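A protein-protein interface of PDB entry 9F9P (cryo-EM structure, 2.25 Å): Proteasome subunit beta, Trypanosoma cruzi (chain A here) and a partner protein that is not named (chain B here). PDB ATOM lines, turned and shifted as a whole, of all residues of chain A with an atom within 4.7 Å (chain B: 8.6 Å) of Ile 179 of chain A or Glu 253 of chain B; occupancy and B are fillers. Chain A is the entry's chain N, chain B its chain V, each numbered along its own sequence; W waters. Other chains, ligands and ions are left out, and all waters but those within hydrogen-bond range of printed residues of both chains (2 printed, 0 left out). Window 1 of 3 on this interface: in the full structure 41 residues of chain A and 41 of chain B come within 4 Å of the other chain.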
ATOM      1  N   ASP A  21      -6.776   8.739 -36.481  1.00  0.00           N
ATOM      2  CA  ASP A  21      -6.280   8.378 -35.162  1.00  0.00           C
ATOM      3  C   ASP A  21      -6.742   6.972 -34.774  1.00  0.00           C
ATOM      4  O   ASP A  21      -7.639   6.420 -35.418  1.00  0.00           O
ATOM      5  CB  ASP A  21      -6.738   9.422 -34.163  1.00  0.00           C
ATOM      6  CG  ASP A  21      -8.188   9.262 -33.742  1.00  0.00           C
ATOM      7  OD1 ASP A  21      -8.797   8.173 -34.091  1.00  0.00           O
ATOM      8  OD2 ASP A  21      -8.729  10.218 -33.036  1.00  0.00           O
ATOM      9  N   THR A  22      -6.151   6.381 -33.739  1.00  0.00           N
ATOM     10  CA  THR A  22      -6.474   5.027 -33.372  1.00  0.00           C
ATOM     11  C   THR A  22      -7.574   4.924 -32.311  1.00  0.00           C
ATOM     12  O   THR A  22      -7.500   4.061 -31.469  1.00  0.00           O
ATOM     13  CB  THR A  22      -5.194   4.341 -32.909  1.00  0.00           C
ATOM     14  OG1 THR A  22      -4.735   4.953 -31.697  1.00  0.00           O
ATOM     15  CG2 THR A  22      -4.151   4.391 -34.020  1.00  0.00           C
ATOM     16  N   LEU A  23      -8.573   5.788 -32.290  1.00  0.00           N
ATOM     17  CA  LEU A  23      -9.484   5.784 -31.159  1.00  0.00           C
ATOM     18  C   LEU A  23     -10.923   5.490 -31.553  1.00  0.00           C
ATOM     19  O   LEU A  23     -11.420   6.070 -32.483  1.00  0.00           O
ATOM     20  CB  LEU A  23      -9.374   7.152 -30.490  1.00  0.00           C
ATOM     21  CG  LEU A  23     -10.423   7.468 -29.416  1.00  0.00           C
ATOM     22  CD1 LEU A  23     -10.184   6.723 -28.085  1.00  0.00           C
ATOM     23  CD2 LEU A  23     -10.497   8.961 -29.209  1.00  0.00           C
ATOM     24  N   PRO A  33      -8.232   3.004 -27.147  1.00  0.00           N
ATOM     25  CA  PRO A  33      -7.268   3.851 -27.825  1.00  0.00           C
ATOM     26  C   PRO A  33      -6.315   3.168 -28.793  1.00  0.00           C
ATOM     27  O   PRO A  33      -5.442   3.824 -29.319  1.00  0.00           O
ATOM     28  CB  PRO A  33      -6.477   4.406 -26.630  1.00  0.00           C
ATOM     29  CG  PRO A  33      -6.503   3.276 -25.620  1.00  0.00           C
ATOM     30  CD  PRO A  33      -7.858   2.628 -25.781  1.00  0.00           C
ATOM     31  N   PHE A 172      -5.973  17.599 -32.603  1.00  0.00           N
ATOM     32  CA  PHE A 172      -5.744  17.252 -31.222  1.00  0.00           C
ATOM     33  C   PHE A 172      -5.964  18.440 -30.275  1.00  0.00           C
ATOM     34  O   PHE A 172      -6.477  18.253 -29.172  1.00  0.00           O
ATOM     35  CB  PHE A 172      -4.341  16.668 -31.073  1.00  0.00           C
ATOM     36  CG  PHE A 172      -3.990  16.298 -29.663  1.00  0.00           C
ATOM     37  CD1 PHE A 172      -4.731  15.352 -28.967  1.00  0.00           C
ATOM     38  CD2 PHE A 172      -2.941  16.940 -29.001  1.00  0.00           C
ATOM     39  CE1 PHE A 172      -4.417  15.061 -27.639  1.00  0.00           C
ATOM     40  CE2 PHE A 172      -2.648  16.657 -27.666  1.00  0.00           C
ATOM     41  CZ  PHE A 172      -3.357  15.691 -26.995  1.00  0.00           C
ATOM     42  N   ALA A 178     -10.580  13.010 -29.244  1.00  0.00           N
ATOM     43  CA  ALA A 178      -9.363  12.736 -30.005  1.00  0.00           C
ATOM     44  C   ALA A 178      -8.253  12.284 -29.062  1.00  0.00           C
ATOM     45  O   ALA A 178      -8.403  12.424 -27.854  1.00  0.00           O
ATOM     46  CB  ALA A 178      -8.959  13.962 -30.810  1.00  0.00           C
ATOM     47  N   ILE A 179      -7.217  11.627 -29.603  1.00  0.00           N
ATOM     48  CA  ILE A 179      -5.979  11.338 -28.889  1.00  0.00           C
ATOM     49  C   ILE A 179      -4.804  11.658 -29.780  1.00  0.00           C
ATOM     50  O   ILE A 179      -4.922  11.660 -30.992  1.00  0.00           O
ATOM     51  CB  ILE A 179      -5.785   9.861 -28.484  1.00  0.00           C
ATOM     52  CG1 ILE A 179      -5.938   8.893 -29.651  1.00  0.00           C
ATOM     53  CG2 ILE A 179      -6.651   9.447 -27.324  1.00  0.00           C
ATOM     54  CD1 ILE A 179      -5.787   7.481 -29.153  1.00  0.00           C
ATOM     55  N   ASN A 180      -3.635  11.734 -29.179  1.00  0.00           N
ATOM     56  CA  ASN A 180      -2.449  12.029 -29.956  1.00  0.00           C
ATOM     57  C   ASN A 180      -1.770  10.731 -30.378  1.00  0.00           C
ATOM     58  O   ASN A 180      -0.713  10.381 -29.904  1.00  0.00           O
ATOM     59  CB  ASN A 180      -1.516  12.942 -29.156  1.00  0.00           C
ATOM     60  CG  ASN A 180      -0.377  13.485 -29.993  1.00  0.00           C
ATOM     61  OD1 ASN A 180      -0.228  13.176 -31.168  1.00  0.00           O
ATOM     62  ND2 ASN A 180       0.419  14.339 -29.404  1.00  0.00           N
ATOM     63  N   LYS A 181      -2.358  10.039 -31.335  1.00  0.00           N
ATOM     64  CA  LYS A 181      -1.819   8.767 -31.807  1.00  0.00           C
ATOM     65  C   LYS A 181      -2.426   8.483 -33.172  1.00  0.00           C
ATOM     66  O   LYS A 181      -3.617   8.249 -33.243  1.00  0.00           O
ATOM     67  CB  LYS A 181      -2.158   7.686 -30.788  1.00  0.00           C
ATOM     68  CG  LYS A 181      -1.565   6.325 -31.104  1.00  0.00           C
ATOM     69  CD  LYS A 181      -1.556   5.511 -29.849  1.00  0.00           C
ATOM     70  CE  LYS A 181      -1.777   4.028 -30.034  1.00  0.00           C
ATOM     71  NZ  LYS A 181      -1.618   3.360 -28.728  1.00  0.00           N
ATOM     72  N   PHE A 182      -1.625   8.536 -34.235  1.00  0.00           N
ATOM     73  CA  PHE A 182      -2.160   8.551 -35.590  1.00  0.00           C
ATOM     74  C   PHE A 182      -1.483   7.520 -36.471  1.00  0.00           C
ATOM     75  O   PHE A 182      -0.321   7.261 -36.277  1.00  0.00           O
ATOM     76  CB  PHE A 182      -1.902   9.931 -36.210  1.00  0.00           C
ATOM     77  CG  PHE A 182      -2.503  11.079 -35.430  1.00  0.00           C
ATOM     78  CD1 PHE A 182      -3.860  11.357 -35.524  1.00  0.00           C
ATOM     79  CD2 PHE A 182      -1.714  11.830 -34.554  1.00  0.00           C
ATOM     80  CE1 PHE A 182      -4.410  12.402 -34.805  1.00  0.00           C
ATOM     81  CE2 PHE A 182      -2.267  12.859 -33.809  1.00  0.00           C
ATOM     82  CZ  PHE A 182      -3.622  13.124 -33.905  1.00  0.00           C
ATOM     83  N   ARG B  73     -10.005  22.844 -19.994  1.00  0.00           N
ATOM     84  CA  ARG B  73     -10.743  22.845 -21.248  1.00  0.00           C
ATOM     85  C   ARG B  73     -12.145  23.427 -21.119  1.00  0.00           C
ATOM     86  O   ARG B  73     -12.891  23.018 -20.254  1.00  0.00           O
ATOM     87  CB  ARG B  73     -10.880  21.383 -21.670  1.00  0.00           C
ATOM     88  CG  ARG B  73     -11.541  21.195 -23.016  1.00  0.00           C
ATOM     89  CD  ARG B  73     -11.452  19.772 -23.556  1.00  0.00           C
ATOM     90  NE  ARG B  73     -10.190  19.541 -24.224  1.00  0.00           N
ATOM     91  CZ  ARG B  73      -9.908  18.403 -24.814  1.00  0.00           C
ATOM     92  NH1 ARG B  73     -10.840  17.472 -24.873  1.00  0.00           N
ATOM     93  NH2 ARG B  73      -8.725  18.222 -25.348  1.00  0.00           N
ATOM     94  N   ALA B 215      -5.009  13.654 -14.221  1.00  0.00           N
ATOM     95  CA  ALA B 215      -4.573  13.028 -15.460  1.00  0.00           C
ATOM     96  C   ALA B 215      -5.380  11.786 -15.808  1.00  0.00           C
ATOM     97  O   ALA B 215      -5.786  11.625 -16.951  1.00  0.00           O
ATOM     98  CB  ALA B 215      -3.095  12.730 -15.390  1.00  0.00           C
ATOM     99  N   TYR B 218      -8.810  12.950 -17.127  1.00  0.00           N
ATOM    100  CA  TYR B 218      -8.912  13.546 -18.441  1.00  0.00           C
ATOM    101  C   TYR B 218      -8.485  12.604 -19.572  1.00  0.00           C
ATOM    102  O   TYR B 218      -8.908  12.853 -20.706  1.00  0.00           O
ATOM    103  CB  TYR B 218      -8.344  14.970 -18.540  1.00  0.00           C
ATOM    104  CG  TYR B 218      -6.869  15.241 -18.562  1.00  0.00           C
ATOM    105  CD1 TYR B 218      -5.941  14.332 -19.002  1.00  0.00           C
ATOM    106  CD2 TYR B 218      -6.416  16.499 -18.229  1.00  0.00           C
ATOM    107  CE1 TYR B 218      -4.586  14.642 -19.031  1.00  0.00           C
ATOM    108  CE2 TYR B 218      -5.068  16.836 -18.285  1.00  0.00           C
ATOM    109  CZ  TYR B 218      -4.141  15.881 -18.634  1.00  0.00           C
ATOM    110  OH  TYR B 218      -2.809  16.176 -18.677  1.00  0.00           O
ATOM    111  N   SER B 219      -7.754  11.532 -19.292  1.00  0.00           N
ATOM    112  CA  SER B 219      -7.453  10.576 -20.342  1.00  0.00           C
ATOM    113  C   SER B 219      -8.692   9.794 -20.779  1.00  0.00           C
ATOM    114  O   SER B 219      -8.791   9.460 -21.933  1.00  0.00           O
ATOM    115  CB  SER B 219      -6.311   9.695 -19.929  1.00  0.00           C
ATOM    116  OG  SER B 219      -5.125  10.523 -19.709  1.00  0.00           O
ATOM    117  N   ARG B 220      -9.725   9.663 -19.955  1.00  0.00           N
ATOM    118  CA  ARG B 220     -10.917   8.925 -20.336  1.00  0.00           C
ATOM    119  C   ARG B 220     -12.100   9.806 -20.714  1.00  0.00           C
ATOM    120  O   ARG B 220     -13.011   9.278 -21.321  1.00  0.00           O
ATOM    121  CB  ARG B 220     -11.313   7.970 -19.197  1.00  0.00           C
ATOM    122  CG  ARG B 220     -10.364   6.786 -19.030  1.00  0.00           C
ATOM    123  CD  ARG B 220     -10.518   5.826 -20.201  1.00  0.00           C
ATOM    124  NE  ARG B 220      -9.674   4.661 -20.093  1.00  0.00           N
ATOM    125  CZ  ARG B 220      -9.743   3.587 -20.877  1.00  0.00           C
ATOM    126  NH1 ARG B 220     -10.618   3.499 -21.867  1.00  0.00           N
ATOM    127  NH2 ARG B 220      -8.897   2.605 -20.663  1.00  0.00           N
ATOM    128  N   TRP B 245       0.415  19.445 -20.983  1.00  0.00           N
ATOM    129  CA  TRP B 245       0.028  18.112 -21.437  1.00  0.00           C
ATOM    130  C   TRP B 245       1.256  17.248 -21.734  1.00  0.00           C
ATOM    131  O   TRP B 245       1.260  16.084 -21.369  1.00  0.00           O
ATOM    132  CB  TRP B 245      -0.932  18.129 -22.657  1.00  0.00           C
ATOM    133  CG  TRP B 245      -1.419  16.739 -22.969  1.00  0.00           C
ATOM    134  CD1 TRP B 245      -2.386  16.036 -22.284  1.00  0.00           C
ATOM    135  CD2 TRP B 245      -0.818  15.802 -23.894  1.00  0.00           C
ATOM    136  NE1 TRP B 245      -2.461  14.750 -22.771  1.00  0.00           N
ATOM    137  CE2 TRP B 245      -1.525  14.586 -23.765  1.00  0.00           C
ATOM    138  CE3 TRP B 245       0.189  15.906 -24.854  1.00  0.00           C
ATOM    139  CZ2 TRP B 245      -1.233  13.471 -24.546  1.00  0.00           C
ATOM    140  CZ3 TRP B 245       0.478  14.817 -25.648  1.00  0.00           C
ATOM    141  CH2 TRP B 245      -0.202  13.599 -25.468  1.00  0.00           C
ATOM    142  N   THR B 248       2.436  15.459 -18.611  1.00  0.00           N
ATOM    143  CA  THR B 248       1.386  14.891 -17.782  1.00  0.00           C
ATOM    144  C   THR B 248       1.915  13.616 -17.127  1.00  0.00           C
ATOM    145  O   THR B 248       2.681  12.893 -17.735  1.00  0.00           O
ATOM    146  CB  THR B 248       0.095  14.723 -18.619  1.00  0.00           C
ATOM    147  OG1 THR B 248      -1.013  14.362 -17.798  1.00  0.00           O
ATOM    148  CG2 THR B 248       0.190  13.674 -19.711  1.00  0.00           C
ATOM    149  N   TYR B 250       0.173  10.867 -16.419  1.00  0.00           N
ATOM    150  CA  TYR B 250      -0.430   9.701 -17.051  1.00  0.00           C
ATOM    151  C   TYR B 250      -1.155  10.107 -18.332  1.00  0.00           C
ATOM    152  O   TYR B 250      -1.898  11.098 -18.344  1.00  0.00           O
ATOM    153  CB  TYR B 250      -1.476   9.025 -16.152  1.00  0.00           C
ATOM    154  CG  TYR B 250      -2.103   7.809 -16.776  1.00  0.00           C
ATOM    155  CD1 TYR B 250      -1.427   6.600 -16.790  1.00  0.00           C
ATOM    156  CD2 TYR B 250      -3.292   7.901 -17.506  1.00  0.00           C
ATOM    157  CE1 TYR B 250      -1.952   5.486 -17.442  1.00  0.00           C
ATOM    158  CE2 TYR B 250      -3.805   6.806 -18.202  1.00  0.00           C
ATOM    159  CZ  TYR B 250      -3.134   5.590 -18.169  1.00  0.00           C
ATOM    160  OH  TYR B 250      -3.642   4.483 -18.837  1.00  0.00           O
ATOM    161  N   CYS B 251      -1.002   9.299 -19.396  1.00  0.00           N
ATOM    162  CA  CYS B 251      -1.945   9.334 -20.525  1.00  0.00           C
ATOM    163  C   CYS B 251      -1.992   7.965 -21.212  1.00  0.00           C
ATOM    164  O   CYS B 251      -1.019   7.224 -21.144  1.00  0.00           O
ATOM    165  CB  CYS B 251      -1.535  10.420 -21.536  1.00  0.00           C
ATOM    166  SG  CYS B 251       0.173  10.180 -22.095  1.00  0.00           S
ATOM    167  N   MET B 252      -3.064   7.676 -21.952  1.00  0.00           N
ATOM    168  CA  MET B 252      -3.179   6.376 -22.612  1.00  0.00           C
ATOM    169  C   MET B 252      -2.131   6.217 -23.714  1.00  0.00           C
ATOM    170  O   MET B 252      -1.578   5.127 -23.849  1.00  0.00           O
ATOM    171  CB  MET B 252      -4.590   6.136 -23.162  1.00  0.00           C
ATOM    172  CG  MET B 252      -5.575   5.859 -22.031  1.00  0.00           C
ATOM    173  SD  MET B 252      -7.251   5.387 -22.493  1.00  0.00           S
ATOM    174  CE  MET B 252      -7.683   6.678 -23.662  1.00  0.00           C
ATOM    175  N   GLU B 253      -1.827   7.314 -24.422  1.00  0.00           N
ATOM    176  CA  GLU B 253      -0.941   7.351 -25.579  1.00  0.00           C
ATOM    177  C   GLU B 253       0.466   6.871 -25.244  1.00  0.00           C
ATOM    178  O   GLU B 253       1.181   6.488 -26.158  1.00  0.00           O
ATOM    179  CB  GLU B 253      -0.755   8.767 -26.142  1.00  0.00           C
ATOM    180  CG  GLU B 253      -1.997   9.481 -26.721  1.00  0.00           C
ATOM    181  CD  GLU B 253      -2.882  10.302 -25.769  1.00  0.00           C
ATOM    182  OE1 GLU B 253      -2.998   9.878 -24.580  1.00  0.00           O
ATOM    183  OE2 GLU B 253      -3.521  11.316 -26.209  1.00  0.00           O
ATOM    184  N   LYS B 254       0.895   6.911 -23.978  1.00  0.00           N
ATOM    185  CA  LYS B 254       2.255   6.527 -23.609  1.00  0.00           C
ATOM    186  C   LYS B 254       2.295   5.340 -22.647  1.00  0.00           C
ATOM    187  O   LYS B 254       3.371   4.904 -22.254  1.00  0.00           O
ATOM    188  CB  LYS B 254       2.997   7.713 -22.980  1.00  0.00           C
ATOM    189  CG  LYS B 254       3.578   8.708 -23.975  1.00  0.00           C
ATOM    190  CD  LYS B 254       3.674  10.139 -23.466  1.00  0.00           C
ATOM    191  CE  LYS B 254       4.270  11.075 -24.502  1.00  0.00           C
ATOM    192  NZ  LYS B 254       3.727  12.456 -24.416  1.00  0.00           N
ATOM    193  N   ASP B 255       1.129   4.809 -22.285  1.00  0.00           N
ATOM    194  CA  ASP B 255       1.005   3.606 -21.477  1.00  0.00           C
ATOM    195  C   ASP B 255       1.380   2.392 -22.335  1.00  0.00           C
ATOM    196  O   ASP B 255       0.788   2.190 -23.398  1.00  0.00           O
ATOM    197  CB  ASP B 255      -0.432   3.495 -20.963  1.00  0.00           C
ATOM    198  CG  ASP B 255      -0.676   2.414 -19.921  1.00  0.00           C
ATOM    199  OD1 ASP B 255       0.271   1.621 -19.638  1.00  0.00           O
ATOM    200  OD2 ASP B 255      -1.803   2.401 -19.362  1.00  0.00           O
ATOM    201  N   PRO B 256       2.375   1.561 -21.944  1.00  0.00           N
ATOM    202  CA  PRO B 256       2.813   0.438 -22.782  1.00  0.00           C
ATOM    203  C   PRO B 256       1.796  -0.684 -23.012  1.00  0.00           C
ATOM    204  O   PRO B 256       1.912  -1.388 -24.008  1.00  0.00           O
ATOM    205  CB  PRO B 256       4.037  -0.122 -22.029  1.00  0.00           C
ATOM    206  CG  PRO B 256       4.468   1.015 -21.106  1.00  0.00           C
ATOM    207  CD  PRO B 256       3.163   1.670 -20.700  1.00  0.00           C
ATOM    208  N   LYS B 257       0.781  -0.825 -22.156  1.00  0.00           N
ATOM    209  CA  LYS B 257      -0.251  -1.820 -22.394  1.00  0.00           C
ATOM    210  C   LYS B 257      -1.229  -1.435 -23.514  1.00  0.00           C
ATOM    211  O   LYS B 257      -2.072  -2.253 -23.877  1.00  0.00           O
ATOM    212  CB  LYS B 257      -1.025  -2.161 -21.116  1.00  0.00           C
ATOM    213  CG  LYS B 257      -1.934  -1.086 -20.531  1.00  0.00           C
ATOM    214  CD  LYS B 257      -2.782  -1.630 -19.366  1.00  0.00           C
ATOM    215  CE  LYS B 257      -3.511  -0.585 -18.532  1.00  0.00           C
ATOM    216  NZ  LYS B 257      -2.616   0.042 -17.522  1.00  0.00           N
ATOM    217  N   TYR B 258      -1.122  -0.228 -24.079  1.00  0.00           N
ATOM    218  CA  TYR B 258      -1.975   0.190 -25.181  1.00  0.00           C
ATOM    219  C   TYR B 258      -1.136   0.534 -26.410  1.00  0.00           C
ATOM    220  O   TYR B 258      -1.625   1.195 -27.313  1.00  0.00           O
ATOM    221  CB  TYR B 258      -2.813   1.429 -24.823  1.00  0.00           C
ATOM    222  CG  TYR B 258      -3.749   1.272 -23.655  1.00  0.00           C
ATOM    223  CD1 TYR B 258      -4.719   0.268 -23.637  1.00  0.00           C
ATOM    224  CD2 TYR B 258      -3.662   2.118 -22.561  1.00  0.00           C
ATOM    225  CE1 TYR B 258      -5.595   0.133 -22.566  1.00  0.00           C
ATOM    226  CE2 TYR B 258      -4.503   1.976 -21.469  1.00  0.00           C
ATOM    227  CZ  TYR B 258      -5.469   0.974 -21.466  1.00  0.00           C
ATOM    228  OH  TYR B 258      -6.281   0.817 -20.372  1.00  0.00           O
ATOM    229  N   ARG B 259       0.118   0.093 -26.457  1.00  0.00           N
ATOM    230  CA  ARG B 259       0.958   0.383 -27.605  1.00  0.00           C
ATOM    231  C   ARG B 259       0.557  -0.482 -28.811  1.00  0.00           C
ATOM    232  O   ARG B 259       0.353   0.042 -29.902  1.00  0.00           O
ATOM    233  CB  ARG B 259       2.425   0.184 -27.224  1.00  0.00           C
ATOM    234  CG  ARG B 259       3.391   0.873 -28.179  1.00  0.00           C
ATOM    235  CD  ARG B 259       4.853   0.688 -27.790  1.00  0.00           C
ATOM    236  NE  ARG B 259       5.174  -0.695 -27.436  1.00  0.00           N
ATOM    237  CZ  ARG B 259       5.051  -1.748 -28.247  1.00  0.00           C
ATOM    238  NH1 ARG B 259       4.708  -1.587 -29.514  1.00  0.00           N
ATOM    239  NH2 ARG B 259       5.284  -2.967 -27.788  1.00  0.00           N
ATOM    240  N   LEU B 261      -1.630  -2.550 -31.402  1.00  0.00           N
ATOM    241  CA  LEU B 261      -2.992  -2.386 -31.865  1.00  0.00           C
ATOM    242  C   LEU B 261      -3.747  -3.702 -31.818  1.00  0.00           C
ATOM    243  O   LEU B 261      -3.196  -4.742 -32.091  1.00  0.00           O
ATOM    244  CB  LEU B 261      -2.963  -1.841 -33.289  1.00  0.00           C
ATOM    245  CG  LEU B 261      -2.322  -0.464 -33.458  1.00  0.00           C
ATOM    246  CD1 LEU B 261      -2.180  -0.107 -34.916  1.00  0.00           C
ATOM    247  CD2 LEU B 261      -3.141   0.622 -32.771  1.00  0.00           C
HETATM  248  O   HOH W   1      -5.655  18.733 -26.330  1.00  0.00           O
HETATM  249  O   HOH W   2      -8.447  16.663 -28.119  1.00  0.00           O
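Of the printed residues of chain B, Pro 33 of chain A touches Met 252 (3.8 Å) and Tyr 258 (3.9 Å).
Of the printed residues of chain B, Phe 172 of chain A touches Trp 245.
Ile 179 of chain A touches just one residue of chain B: Glu 253.
Of the printed residues of chain B, Asn 180 of chain A touches Trp 245 and Glu 253.
Of the printed residues of chain A, Trp 245 of chain B touches Phe 172 (3.9 Å) and Asn 180 (3.8 Å).
Printed residues of chain A within 4 Å of Glu 253 of chain B: Ile 179 (3.5 Å) and Asn 180 (3.0 Å).
Of the printed residues of chain A, Tyr 258 of chain B touches Pro 33 (3.9 Å) and Lys 181 (2.6 Å).
Arg 259 of chain B touches none of the printed residues of chain A.
The nearest residue of chain B that does not touch Ile 179 of chain A is Met 252 of chain B (4.7 Å).
The nearest residue of chain A that does not touch Glu 253 of chain B is Phe 172 of chain A (4.1 Å).
Along chain B the printed residues that touch a printed residue of chain A span positions 245 to 258.
Printed residues of chain A that touch a printed residue of chain B: Pro 33, Phe 172, Ile 179, Asn 180 and Lys 181.
Hydrophobic or aromatic side chains of chain A within 4 Å of the printed part of chain B: Pro 33, Phe 172 and Ile 179.
Among the printed residues, 7 pairs touch across the chains.
Water W2 bridges O of Phe 172 of chain A and NH2 of Arg 73 of chain B.
Water W1 lies within hydrogen-bond range of O of Phe 172 of chain A (3.0 Å) and NH2 of Arg 73 of chain B (3.3 Å).
OG1 of Thr 22 of chain A is in hydrogen-bond range of O of Pro 33 of chain A (2.7 Å).
O of Lys 181 of chain A sits at hydrogen-bond distance from N of Thr 22 of chain A (3.2 Å).
The guanidinium group of Arg 220 of chain B sits close to the side-chain sulfur of Met 252 of chain B, at 3.5 Å.
The guanidinium group of Arg 220 of chain B sits at hydrogen-bond distance from the side-chain hydroxyl of Tyr 258 of chain B.
OE2 of Glu 253 of chain B lies within hydrogen-bond range of N of Asn 180 of chain A (3.0 Å).
O of Tyr 258 of chain B lies within hydrogen-bond range of NZ of Lys 181 of chain A (2.6 Å).
Pro 33 of chain A touches Met 252 of chain B.
CG of Pro 33 of chain A touches CG of Tyr 258 of chain B (3.9 Å).
CZ of Phe 172 of chain A touches CE2 of Trp 245 of chain B, at 3.9 Å.
Ile 179 of chain A touches Glu 253 of chain B (CB to OE2, 3.5 Å).
Trp 245 of chain B touches Asn 180 of chain A (CZ3 to ND2, 3.8 Å).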
